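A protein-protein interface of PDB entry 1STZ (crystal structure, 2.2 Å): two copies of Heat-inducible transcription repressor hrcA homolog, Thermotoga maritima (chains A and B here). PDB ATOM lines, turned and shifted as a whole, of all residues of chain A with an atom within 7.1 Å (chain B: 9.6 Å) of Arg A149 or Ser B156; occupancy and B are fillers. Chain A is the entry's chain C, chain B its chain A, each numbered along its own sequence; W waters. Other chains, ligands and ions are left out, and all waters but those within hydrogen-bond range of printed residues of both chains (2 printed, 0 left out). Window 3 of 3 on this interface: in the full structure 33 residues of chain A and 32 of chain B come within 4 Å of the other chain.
Water W2 bridges the backbone carbonyl oxygen of Thr A166 (2.6 Å) and the side-chain hydroxyl of Tyr B159 (2.9 Å).
Water W1 bridges the backbone carbonyl oxygen of Val B155 (2.6 Å) and the guanidinium group of Arg A149 (3.0 Å).
Of the 17 printed residues of chain B, 4 touch a printed residue of chain A.
Hydrophobic or aromatic side chains of chain A that line the printed part of chain B: Ile A153, Leu A165 and Val A170.
Among the printed residues, 6 pairs touch across the chains.
The backbone carbonyl oxygen (O) of Ile B161 is in hydrogen-bond range of the backbone NH (N) of Ile B153 (2.8 Å).
N of Asp B158 sits close to OG of Ser B156 (3.2 Å).
OG of Ser B156 sits at hydrogen-bond distance from N of Tyr B159, at 3.4 Å.
The backbone NH (N) of Leu A148 lies within hydrogen-bond range of the backbone carbonyl oxygen (O) of Leu A165.
The backbone carbonyl oxygen of Arg A149 lies within hydrogen-bond range of the backbone NH of Leu A165, 2.9 Å away.
Ile A153 touches its own counterpart, Ile B153.
1 position is printed for both chains.
Of the 6 pairs that touch across the chains among the printed residues, 1 has its exchanged pair printed and touching as well.
The backbone carbonyl oxygen (O) of Val B155 lies within hydrogen-bond range of the guanidinium group (NH1) of Arg A149 (2.8 Å).
Of chain B, only Val B155 (2.8 Å) and Ser B156 (3.9 Å) come within 4 Å of Arg A149.
No residue of chain B comes within 4 Å of Val A150.
Of the printed residues of chain B, Ile A153 touches Ile B153 (3.8 Å) and Val B155 (3.5 Å).
Of the printed residues of chain B, Leu A165 touches Tyr B159 (3.6 Å).
Of the printed residues of chain B, Val A170 touches Tyr B159 (3.8 Å).
Glu A188 touches none of the printed residues of chain B.
Printed residues of chain A within 4 Å of Ile B153: Ile A153.
Ser B156 touches one residue of chain A.
Of the printed residues of chain A, Tyr B159 touches Leu A165 and Val A170.
Leu B160 touches none of the printed residues of chain A.
The nearest residue of chain B that does not touch Arg A149 is Pro B154 (6.1 Å).
The nearest residue of chain A that does not touch Ser B156 is Leu A165 (5.0 Å).
The nearest printed residue of chain B that does not touch Ile A153 is Ile B161 (4.3 Å).
Among the printed residues, merely in contact across the chains: Arg A149 with Ser B156, Ile A153 with Ile B153, Ile A153 with Val B155, Leu A165 with Tyr B159 and Val A170 with Tyr B159.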
ATOM      1  N   LYS A 146      17.976 -42.672 -17.562  1.00  0.00           N
ATOM      2  CA  LYS A 146      18.753 -41.653 -16.861  1.00  0.00           C
ATOM      3  C   LYS A 146      18.341 -40.234 -17.260  1.00  0.00           C
ATOM      4  O   LYS A 146      18.192 -39.933 -18.437  1.00  0.00           O
ATOM      5  CB  LYS A 146      20.254 -41.826 -17.121  1.00  0.00           C
ATOM      6  CG  LYS A 146      20.992 -42.612 -16.047  1.00  0.00           C
ATOM      7  CD  LYS A 146      22.500 -42.528 -16.238  1.00  0.00           C
ATOM      8  CE  LYS A 146      23.241 -43.213 -15.102  1.00  0.00           C
ATOM      9  NZ  LYS A 146      22.745 -44.600 -14.849  1.00  0.00           N
ATOM     10  N   ILE A 147      18.145 -39.376 -16.259  1.00  0.00           N
ATOM     11  CA  ILE A 147      17.982 -37.947 -16.476  1.00  0.00           C
ATOM     12  C   ILE A 147      19.380 -37.390 -16.718  1.00  0.00           C
ATOM     13  O   ILE A 147      20.227 -37.444 -15.834  1.00  0.00           O
ATOM     14  CB  ILE A 147      17.359 -37.271 -15.247  1.00  0.00           C
ATOM     15  CG1 ILE A 147      15.947 -37.796 -15.011  1.00  0.00           C
ATOM     16  CG2 ILE A 147      17.350 -35.767 -15.435  1.00  0.00           C
ATOM     17  CD1 ILE A 147      15.366 -37.440 -13.662  1.00  0.00           C
ATOM     18  N   LEU A 148      19.624 -36.896 -17.925  1.00  0.00           N
ATOM     19  CA  LEU A 148      20.929 -36.342 -18.294  1.00  0.00           C
ATOM     20  C   LEU A 148      21.036 -34.857 -17.921  1.00  0.00           C
ATOM     21  O   LEU A 148      22.133 -34.334 -17.715  1.00  0.00           O
ATOM     22  CB  LEU A 148      21.162 -36.519 -19.793  1.00  0.00           C
ATOM     23  CG  LEU A 148      21.131 -37.972 -20.280  1.00  0.00           C
ATOM     24  CD1 LEU A 148      21.022 -38.044 -21.786  1.00  0.00           C
ATOM     25  CD2 LEU A 148      22.374 -38.727 -19.794  1.00  0.00           C
ATOM     26  N   ARG A 149      19.888 -34.181 -17.848  1.00  0.00           N
ATOM     27  CA  ARG A 149      19.856 -32.744 -17.586  1.00  0.00           C
ATOM     28  C   ARG A 149      18.461 -32.223 -17.271  1.00  0.00           C
ATOM     29  O   ARG A 149      17.490 -32.654 -17.877  1.00  0.00           O
ATOM     30  CB  ARG A 149      20.355 -32.018 -18.821  1.00  0.00           C
ATOM     31  CG  ARG A 149      20.677 -30.592 -18.608  1.00  0.00           C
ATOM     32  CD  ARG A 149      21.339 -29.992 -19.809  1.00  0.00           C
ATOM     33  NE  ARG A 149      21.030 -28.575 -19.912  1.00  0.00           N
ATOM     34  CZ  ARG A 149      21.072 -27.884 -21.041  1.00  0.00           C
ATOM     35  NH1 ARG A 149      21.413 -28.480 -22.178  1.00  0.00           N
ATOM     36  NH2 ARG A 149      20.772 -26.587 -21.026  1.00  0.00           N
ATOM     37  N   VAL A 150      18.371 -31.287 -16.336  1.00  0.00           N
ATOM     38  CA  VAL A 150      17.116 -30.609 -16.041  1.00  0.00           C
ATOM     39  C   VAL A 150      17.190 -29.152 -16.488  1.00  0.00           C
ATOM     40  O   VAL A 150      18.189 -28.467 -16.240  1.00  0.00           O
ATOM     41  CB  VAL A 150      16.767 -30.673 -14.553  1.00  0.00           C
ATOM     42  CG1 VAL A 150      15.409 -30.016 -14.313  1.00  0.00           C
ATOM     43  CG2 VAL A 150      16.759 -32.120 -14.076  1.00  0.00           C
ATOM     44  N   MET A 151      16.121 -28.684 -17.132  1.00  0.00           N
ATOM     45  CA  MET A 151      16.066 -27.340 -17.691  1.00  0.00           C
ATOM     46  C   MET A 151      14.852 -26.564 -17.226  1.00  0.00           C
ATOM     47  O   MET A 151      13.734 -27.008 -17.416  1.00  0.00           O
ATOM     48  CB  MET A 151      16.038 -27.439 -19.200  1.00  0.00           C
ATOM     49  CG  MET A 151      17.353 -27.953 -19.729  1.00  0.00           C
ATOM     50  SD  MET A 151      17.232 -29.023 -21.097  1.00  0.00           S
ATOM     51  CE  MET A 151      16.474 -30.472 -20.428  1.00  0.00           C
ATOM     52  N   ILE A 153      13.689 -22.788 -18.081  1.00  0.00           N
ATOM     53  CA  ILE A 153      14.015 -21.652 -18.924  1.00  0.00           C
ATOM     54  C   ILE A 153      12.937 -20.583 -18.779  1.00  0.00           C
ATOM     55  O   ILE A 153      11.846 -20.750 -19.301  1.00  0.00           O
ATOM     56  CB  ILE A 153      14.101 -22.088 -20.394  1.00  0.00           C
ATOM     57  CG1 ILE A 153      15.051 -23.278 -20.572  1.00  0.00           C
ATOM     58  CG2 ILE A 153      14.577 -20.914 -21.257  1.00  0.00           C
ATOM     59  CD1 ILE A 153      14.679 -24.155 -21.735  1.00  0.00           C
ATOM     60  N   PHE A 162       9.836 -25.959 -18.302  1.00  0.00           N
ATOM     61  CA  PHE A 162      10.579 -27.035 -17.690  1.00  0.00           C
ATOM     62  C   PHE A 162      10.682 -28.181 -18.686  1.00  0.00           C
ATOM     63  O   PHE A 162       9.728 -28.438 -19.393  1.00  0.00           O
ATOM     64  CB  PHE A 162       9.824 -27.505 -16.458  1.00  0.00           C
ATOM     65  CG  PHE A 162      10.193 -28.878 -16.024  1.00  0.00           C
ATOM     66  CD1 PHE A 162      11.444 -29.124 -15.471  1.00  0.00           C
ATOM     67  CD2 PHE A 162       9.303 -29.936 -16.178  1.00  0.00           C
ATOM     68  CE1 PHE A 162      11.809 -30.411 -15.069  1.00  0.00           C
ATOM     69  CE2 PHE A 162       9.656 -31.235 -15.778  1.00  0.00           C
ATOM     70  CZ  PHE A 162      10.912 -31.467 -15.223  1.00  0.00           C
ATOM     71  N   SER A 163      11.823 -28.870 -18.743  1.00  0.00           N
ATOM     72  CA  SER A 163      11.895 -30.186 -19.373  1.00  0.00           C
ATOM     73  C   SER A 163      13.085 -30.954 -18.832  1.00  0.00           C
ATOM     74  O   SER A 163      13.894 -30.408 -18.078  1.00  0.00           O
ATOM     75  CB  SER A 163      12.009 -30.062 -20.901  1.00  0.00           C
ATOM     76  OG  SER A 163      13.177 -29.338 -21.276  1.00  0.00           O
ATOM     77  N   ILE A 164      13.193 -32.218 -19.216  1.00  0.00           N
ATOM     78  CA  ILE A 164      14.385 -33.003 -18.960  1.00  0.00           C
ATOM     79  C   ILE A 164      14.965 -33.521 -20.260  1.00  0.00           C
ATOM     80  O   ILE A 164      14.267 -33.693 -21.242  1.00  0.00           O
ATOM     81  CB  ILE A 164      14.121 -34.204 -17.992  1.00  0.00           C
ATOM     82  CG1 ILE A 164      13.120 -35.199 -18.581  1.00  0.00           C
ATOM     83  CG2 ILE A 164      13.628 -33.731 -16.629  1.00  0.00           C
ATOM     84  CD1 ILE A 164      13.034 -36.502 -17.784  1.00  0.00           C
ATOM     85  N   LEU A 165      16.258 -33.781 -20.230  1.00  0.00           N
ATOM     86  CA  LEU A 165      16.962 -34.392 -21.323  1.00  0.00           C
ATOM     87  C   LEU A 165      17.170 -35.855 -20.939  1.00  0.00           C
ATOM     88  O   LEU A 165      17.601 -36.165 -19.832  1.00  0.00           O
ATOM     89  CB  LEU A 165      18.307 -33.699 -21.521  1.00  0.00           C
ATOM     90  CG  LEU A 165      18.757 -33.384 -22.936  1.00  0.00           C
ATOM     91  CD1 LEU A 165      20.161 -32.746 -22.882  1.00  0.00           C
ATOM     92  CD2 LEU A 165      18.764 -34.624 -23.811  1.00  0.00           C
ATOM     93  N   THR A 166      16.817 -36.746 -21.852  1.00  0.00           N
ATOM     94  CA  THR A 166      17.119 -38.151 -21.699  1.00  0.00           C
ATOM     95  C   THR A 166      17.748 -38.661 -22.995  1.00  0.00           C
ATOM     96  O   THR A 166      17.906 -37.894 -23.934  1.00  0.00           O
ATOM     97  CB  THR A 166      15.824 -38.889 -21.315  1.00  0.00           C
ATOM     98  OG1 THR A 166      16.150 -40.036 -20.533  1.00  0.00           O
ATOM     99  CG2 THR A 166      15.095 -39.444 -22.504  1.00  0.00           C
ATOM    100  N   VAL A 170      13.989 -34.819 -25.453  1.00  0.00           N
ATOM    101  CA  VAL A 170      13.514 -33.869 -24.476  1.00  0.00           C
ATOM    102  C   VAL A 170      12.110 -34.281 -24.051  1.00  0.00           C
ATOM    103  O   VAL A 170      11.212 -34.316 -24.878  1.00  0.00           O
ATOM    104  CB  VAL A 170      13.478 -32.450 -25.079  1.00  0.00           C
ATOM    105  CG1 VAL A 170      13.069 -31.425 -24.030  1.00  0.00           C
ATOM    106  CG2 VAL A 170      14.825 -32.084 -25.671  1.00  0.00           C
ATOM    107  N   GLU A 188      17.340 -24.444 -10.670  1.00  0.00           N
ATOM    108  CA  GLU A 188      17.867 -25.282 -11.735  1.00  0.00           C
ATOM    109  C   GLU A 188      19.120 -26.031 -11.284  1.00  0.00           C
ATOM    110  O   GLU A 188      19.222 -27.242 -11.509  1.00  0.00           O
ATOM    111  CB  GLU A 188      18.189 -24.455 -12.966  1.00  0.00           C
ATOM    112  CG  GLU A 188      18.588 -25.275 -14.183  1.00  0.00           C
ATOM    113  CD  GLU A 188      18.652 -24.411 -15.426  1.00  0.00           C
ATOM    114  OE1 GLU A 188      19.418 -23.417 -15.403  1.00  0.00           O
ATOM    115  OE2 GLU A 188      17.937 -24.700 -16.405  1.00  0.00           O
ATOM    116  N   ASN A 192      19.505 -30.217 -10.956  1.00  0.00           N
ATOM    117  CA  ASN A 192      20.540 -31.012 -11.610  1.00  0.00           C
ATOM    118  C   ASN A 192      21.431 -31.763 -10.629  1.00  0.00           C
ATOM    119  O   ASN A 192      21.802 -32.907 -10.876  1.00  0.00           O
ATOM    120  CB  ASN A 192      21.374 -30.134 -12.545  1.00  0.00           C
ATOM    121  CG  ASN A 192      20.652 -29.836 -13.840  1.00  0.00           C
ATOM    122  OD1 ASN A 192      20.542 -30.695 -14.700  1.00  0.00           O
ATOM    123  ND2 ASN A 192      20.115 -28.627 -13.967  1.00  0.00           N
ATOM    124  N   LEU A 195      19.080 -34.609  -9.376  1.00  0.00           N
ATOM    125  CA  LEU A 195      18.426 -35.504 -10.341  1.00  0.00           C
ATOM    126  C   LEU A 195      19.290 -36.009 -11.508  1.00  0.00           C
ATOM    127  O   LEU A 195      18.962 -37.023 -12.123  1.00  0.00           O
ATOM    128  CB  LEU A 195      17.185 -34.823 -10.929  1.00  0.00           C
ATOM    129  CG  LEU A 195      16.016 -34.480  -9.996  1.00  0.00           C
ATOM    130  CD1 LEU A 195      14.809 -34.082 -10.807  1.00  0.00           C
ATOM    131  CD2 LEU A 195      15.657 -35.627  -9.066  1.00  0.00           C
ATOM    132  N   ARG A 196      20.369 -35.304 -11.832  1.00  0.00           N
ATOM    133  CA  ARG A 196      21.233 -35.714 -12.935  1.00  0.00           C
ATOM    134  C   ARG A 196      22.003 -37.005 -12.587  1.00  0.00           C
ATOM    135  O   ARG A 196      22.681 -37.061 -11.580  1.00  0.00           O
ATOM    136  CB  ARG A 196      22.203 -34.597 -13.285  1.00  0.00           C
ATOM    137  CG  ARG A 196      22.977 -34.832 -14.554  1.00  0.00           C
ATOM    138  CD  ARG A 196      24.031 -33.774 -14.808  1.00  0.00           C
ATOM    139  NE  ARG A 196      23.433 -32.529 -15.275  1.00  0.00           N
ATOM    140  CZ  ARG A 196      24.097 -31.396 -15.436  1.00  0.00           C
ATOM    141  NH1 ARG A 196      25.392 -31.325 -15.145  1.00  0.00           N
ATOM    142  NH2 ARG A 196      23.471 -30.316 -15.873  1.00  0.00           N
ATOM    143  N   GLY A 197      21.871 -38.029 -13.427  1.00  0.00           N
ATOM    144  CA  GLY A 197      22.464 -39.335 -13.175  1.00  0.00           C
ATOM    145  C   GLY A 197      21.523 -40.317 -12.495  1.00  0.00           C
ATOM    146  O   GLY A 197      21.847 -41.491 -12.342  1.00  0.00           O
ATOM    147  N   ILE B 153      13.999 -21.305 -28.419  1.00  0.00           N
ATOM    148  CA  ILE B 153      15.037 -21.391 -27.373  1.00  0.00           C
ATOM    149  C   ILE B 153      16.035 -22.543 -27.576  1.00  0.00           C
ATOM    150  O   ILE B 153      15.681 -23.691 -27.399  1.00  0.00           O
ATOM    151  CB  ILE B 153      14.339 -21.558 -26.008  1.00  0.00           C
ATOM    152  CG1 ILE B 153      13.451 -20.341 -25.717  1.00  0.00           C
ATOM    153  CG2 ILE B 153      15.354 -21.751 -24.902  1.00  0.00           C
ATOM    154  CD1 ILE B 153      12.021 -20.610 -25.896  1.00  0.00           C
ATOM    155  N   PRO B 154      17.281 -22.266 -27.929  1.00  0.00           N
ATOM    156  CA  PRO B 154      18.275 -23.347 -28.013  1.00  0.00           C
ATOM    157  C   PRO B 154      18.638 -23.901 -26.626  1.00  0.00           C
ATOM    158  O   PRO B 154      19.214 -23.165 -25.831  1.00  0.00           O
ATOM    159  CB  PRO B 154      19.501 -22.680 -28.667  1.00  0.00           C
ATOM    160  CG  PRO B 154      19.105 -21.269 -28.978  1.00  0.00           C
ATOM    161  CD  PRO B 154      17.849 -20.953 -28.273  1.00  0.00           C
ATOM    162  N   VAL B 155      18.291 -25.157 -26.345  1.00  0.00           N
ATOM    163  CA  VAL B 155      18.675 -25.795 -25.081  1.00  0.00           C
ATOM    164  C   VAL B 155      20.020 -26.503 -25.180  1.00  0.00           C
ATOM    165  O   VAL B 155      20.715 -26.623 -24.180  1.00  0.00           O
ATOM    166  CB  VAL B 155      17.597 -26.755 -24.532  1.00  0.00           C
ATOM    167  CG1 VAL B 155      16.322 -25.991 -24.227  1.00  0.00           C
ATOM    168  CG2 VAL B 155      17.312 -27.921 -25.481  1.00  0.00           C
ATOM    169  N   SER B 156      20.403 -26.955 -26.371  1.00  0.00           N
ATOM    170  CA  SER B 156      21.773 -27.433 -26.601  1.00  0.00           C
ATOM    171  C   SER B 156      22.137 -27.365 -28.083  1.00  0.00           C
ATOM    172  O   SER B 156      21.373 -26.828 -28.886  1.00  0.00           O
ATOM    173  CB  SER B 156      21.943 -28.863 -26.068  1.00  0.00           C
ATOM    174  OG  SER B 156      21.164 -29.782 -26.810  1.00  0.00           O
ATOM    175  N   GLU B 157      23.308 -27.899 -28.435  1.00  0.00           N
ATOM    176  CA  GLU B 157      23.696 -28.079 -29.834  1.00  0.00           C
ATOM    177  C   GLU B 157      22.642 -28.897 -30.583  1.00  0.00           C
ATOM    178  O   GLU B 157      22.360 -28.622 -31.748  1.00  0.00           O
ATOM    179  CB  GLU B 157      25.062 -28.783 -29.950  1.00  0.00           C
ATOM    180  CG  GLU B 157      26.273 -27.870 -29.787  1.00  0.00           C
ATOM    181  CD  GLU B 157      27.601 -28.625 -29.773  1.00  0.00           C
ATOM    182  OE1 GLU B 157      27.644 -29.769 -29.269  1.00  0.00           O
ATOM    183  OE2 GLU B 157      28.612 -28.076 -30.264  1.00  0.00           O
ATOM    184  N   ASP B 158      22.053 -29.883 -29.904  1.00  0.00           N
ATOM    185  CA  ASP B 158      21.155 -30.853 -30.533  1.00  0.00           C
ATOM    186  C   ASP B 158      19.675 -30.501 -30.502  1.00  0.00           C
ATOM    187  O   ASP B 158      18.914 -31.017 -31.310  1.00  0.00           O
ATOM    188  CB  ASP B 158      21.332 -32.225 -29.880  1.00  0.00           C
ATOM    189  CG  ASP B 158      22.756 -32.722 -29.951  1.00  0.00           C
ATOM    190  OD1 ASP B 158      23.434 -32.451 -30.966  1.00  0.00           O
ATOM    191  OD2 ASP B 158      23.286 -33.379 -29.033  1.00  0.00           O
ATOM    192  N   TYR B 159      19.258 -29.633 -29.581  1.00  0.00           N
ATOM    193  CA  TYR B 159      17.835 -29.417 -29.342  1.00  0.00           C
ATOM    194  C   TYR B 159      17.411 -27.952 -29.277  1.00  0.00           C
ATOM    195  O   TYR B 159      18.125 -27.096 -28.783  1.00  0.00           O
ATOM    196  CB  TYR B 159      17.419 -30.136 -28.054  1.00  0.00           C
ATOM    197  CG  TYR B 159      17.691 -31.627 -28.067  1.00  0.00           C
ATOM    198  CD1 TYR B 159      18.678 -32.186 -27.258  1.00  0.00           C
ATOM    199  CD2 TYR B 159      16.966 -32.477 -28.891  1.00  0.00           C
ATOM    200  CE1 TYR B 159      18.930 -33.553 -27.271  1.00  0.00           C
ATOM    201  CE2 TYR B 159      17.214 -33.842 -28.912  1.00  0.00           C
ATOM    202  CZ  TYR B 159      18.189 -34.373 -28.100  1.00  0.00           C
ATOM    203  OH  TYR B 159      18.426 -35.723 -28.124  1.00  0.00           O
ATOM    204  N   LEU B 160      16.205 -27.702 -29.760  1.00  0.00           N
ATOM    205  CA  LEU B 160      15.588 -26.385 -29.786  1.00  0.00           C
ATOM    206  C   LEU B 160      14.179 -26.511 -29.240  1.00  0.00           C
ATOM    207  O   LEU B 160      13.505 -27.483 -29.542  1.00  0.00           O
ATOM    208  CB  LEU B 160      15.509 -25.911 -31.240  1.00  0.00           C
ATOM    209  CG  LEU B 160      15.305 -24.432 -31.555  1.00  0.00           C
ATOM    210  CD1 LEU B 160      15.950 -24.079 -32.900  1.00  0.00           C
ATOM    211  CD2 LEU B 160      13.841 -24.071 -31.576  1.00  0.00           C
ATOM    212  N   ILE B 161      13.712 -25.544 -28.458  1.00  0.00           N
ATOM    213  CA  ILE B 161      12.313 -25.536 -28.065  1.00  0.00           C
ATOM    214  C   ILE B 161      11.561 -24.371 -28.692  1.00  0.00           C
ATOM    215  O   ILE B 161      11.904 -23.211 -28.500  1.00  0.00           O
ATOM    216  CB  ILE B 161      12.146 -25.558 -26.518  1.00  0.00           C
ATOM    217  CG1 ILE B 161      12.639 -26.897 -25.964  1.00  0.00           C
ATOM    218  CG2 ILE B 161      10.682 -25.376 -26.155  1.00  0.00           C
ATOM    219  CD1 ILE B 161      12.778 -26.940 -24.462  1.00  0.00           C
ATOM    220  N   ILE B 176      12.601 -29.664 -30.840  1.00  0.00           N
ATOM    221  CA  ILE B 176      12.995 -29.918 -32.226  1.00  0.00           C
ATOM    222  C   ILE B 176      14.445 -30.389 -32.256  1.00  0.00           C
ATOM    223  O   ILE B 176      15.279 -29.835 -31.553  1.00  0.00           O
ATOM    224  CB  ILE B 176      12.854 -28.623 -33.062  1.00  0.00           C
ATOM    225  CG1 ILE B 176      11.403 -28.139 -33.073  1.00  0.00           C
ATOM    226  CG2 ILE B 176      13.306 -28.842 -34.487  1.00  0.00           C
ATOM    227  CD1 ILE B 176      11.285 -26.671 -33.426  1.00  0.00           C
ATOM    228  N   LYS B 177      14.738 -31.417 -33.053  1.00  0.00           N
ATOM    229  CA  LYS B 177      16.120 -31.807 -33.360  1.00  0.00           C
ATOM    230  C   LYS B 177      16.776 -30.802 -34.291  1.00  0.00           C
ATOM    231  O   LYS B 177      16.173 -30.347 -35.257  1.00  0.00           O
ATOM    232  CB  LYS B 177      16.171 -33.154 -34.079  1.00  0.00           C
ATOM    233  CG  LYS B 177      15.767 -34.360 -33.260  1.00  0.00           C
ATOM    234  CD  LYS B 177      16.340 -35.634 -33.877  1.00  0.00           C
ATOM    235  CE  LYS B 177      16.016 -36.850 -33.044  1.00  0.00           C
ATOM    236  NZ  LYS B 177      16.287 -38.109 -33.782  1.00  0.00           N
ATOM    237  N   THR B 178      18.029 -30.480 -34.008  1.00  0.00           N
ATOM    238  CA  THR B 178      18.868 -29.754 -34.950  1.00  0.00           C
ATOM    239  C   THR B 178      20.260 -30.374 -35.013  1.00  0.00           C
ATOM    240  O   THR B 178      21.036 -30.257 -34.065  1.00  0.00           O
ATOM    241  CB  THR B 178      18.976 -28.277 -34.562  1.00  0.00           C
ATOM    242  OG1 THR B 178      17.677 -27.706 -34.400  1.00  0.00           O
ATOM    243  CG2 THR B 178      19.587 -27.482 -35.691  1.00  0.00           C
ATOM    244  N   GLN B 179      20.579 -31.024 -36.131  1.00  0.00           N
ATOM    245  CA  GLN B 179      21.931 -31.565 -36.358  1.00  0.00           C
ATOM    246  C   GLN B 179      22.899 -30.549 -36.974  1.00  0.00           C
ATOM    247  O   GLN B 179      24.113 -30.804 -37.024  1.00  0.00           O
ATOM    248  CB  GLN B 179      21.880 -32.823 -37.238  1.00  0.00           C
ATOM    249  CG  GLN B 179      20.913 -33.924 -36.746  1.00  0.00           C
ATOM    250  CD  GLN B 179      21.329 -34.566 -35.421  1.00  0.00           C
ATOM    251  OE1 GLN B 179      20.517 -34.663 -34.496  1.00  0.00           O
ATOM    252  NE2 GLN B 179      22.578 -35.026 -35.338  1.00  0.00           N
ATOM    253  N   GLU B 180      22.376 -29.418 -37.457  1.00  0.00           N
ATOM    254  CA  GLU B 180      23.227 -28.318 -37.949  1.00  0.00           C
ATOM    255  C   GLU B 180      22.742 -26.949 -37.447  1.00  0.00           C
ATOM    256  O   GLU B 180      21.578 -26.588 -37.626  1.00  0.00           O
ATOM    257  CB  GLU B 180      23.296 -28.321 -39.484  1.00  0.00           C
ATOM    258  CG  GLU B 180      24.113 -29.459 -40.093  1.00  0.00           C
ATOM    259  CD  GLU B 180      25.615 -29.247 -39.999  1.00  0.00           C
ATOM    260  OE1 GLU B 180      26.256 -29.000 -41.046  1.00  0.00           O
ATOM    261  OE2 GLU B 180      26.170 -29.338 -38.882  1.00  0.00           O
ATOM    262  N   ARG B 181      23.652 -26.197 -36.831  1.00  0.00           N
ATOM    263  CA  ARG B 181      23.339 -24.899 -36.226  1.00  0.00           C
ATOM    264  C   ARG B 181      23.050 -23.803 -37.262  1.00  0.00           C
ATOM    265  O   ARG B 181      23.890 -23.507 -38.120  1.00  0.00           O
ATOM    266  CB  ARG B 181      24.499 -24.440 -35.318  1.00  0.00           C
ATOM    267  CG  ARG B 181      24.096 -23.389 -34.279  1.00  0.00           C
ATOM    268  CD  ARG B 181      25.267 -22.792 -33.465  1.00  0.00           C
ATOM    269  NE  ARG B 181      25.630 -23.584 -32.280  1.00  0.00           N
ATOM    270  CZ  ARG B 181      24.866 -23.753 -31.190  1.00  0.00           C
ATOM    271  NH1 ARG B 181      23.658 -23.190 -31.087  1.00  0.00           N
ATOM    272  NH2 ARG B 181      25.316 -24.506 -30.188  1.00  0.00           N
ATOM    273  N   LEU B 182      21.857 -23.215 -37.175  1.00  0.00           N
ATOM    274  CA  LEU B 182      21.534 -21.959 -37.854  1.00  0.00           C
ATOM    275  C   LEU B 182      21.541 -20.855 -36.797  1.00  0.00           C
ATOM    276  O   LEU B 182      21.655 -21.143 -35.604  1.00  0.00           O
ATOM    277  CB  LEU B 182      20.170 -22.040 -38.539  1.00  0.00           C
ATOM    278  CG  LEU B 182      19.899 -23.287 -39.387  1.00  0.00           C
ATOM    279  CD1 LEU B 182      18.439 -23.319 -39.845  1.00  0.00           C
ATOM    280  CD2 LEU B 182      20.838 -23.367 -40.578  1.00  0.00           C
ATOM    281  N   TRP B 184      19.810 -18.804 -34.504  1.00  0.00           N
ATOM    282  CA  TRP B 184      18.472 -18.953 -33.951  1.00  0.00           C
ATOM    283  C   TRP B 184      17.890 -17.624 -33.477  1.00  0.00           C
ATOM    284  O   TRP B 184      16.696 -17.396 -33.602  1.00  0.00           O
ATOM    285  CB  TRP B 184      18.468 -20.007 -32.829  1.00  0.00           C
ATOM    286  CG  TRP B 184      18.947 -21.347 -33.308  1.00  0.00           C
ATOM    287  CD1 TRP B 184      20.056 -22.022 -32.890  1.00  0.00           C
ATOM    288  CD2 TRP B 184      18.350 -22.157 -34.329  1.00  0.00           C
ATOM    289  NE1 TRP B 184      20.187 -23.201 -33.585  1.00  0.00           N
ATOM    290  CE2 TRP B 184      19.145 -23.313 -34.469  1.00  0.00           C
ATOM    291  CE3 TRP B 184      17.215 -22.026 -35.140  1.00  0.00           C
ATOM    292  CZ2 TRP B 184      18.852 -24.320 -35.383  1.00  0.00           C
ATOM    293  CZ3 TRP B 184      16.913 -23.037 -36.040  1.00  0.00           C
ATOM    294  CH2 TRP B 184      17.730 -24.167 -36.154  1.00  0.00           C
HETATM  295  O   HOH W   1      23.266 -26.567 -23.651  1.00  0.00           O
HETATM  296  O   HOH W   2      19.510 -37.056 -25.789  1.00  0.00           O
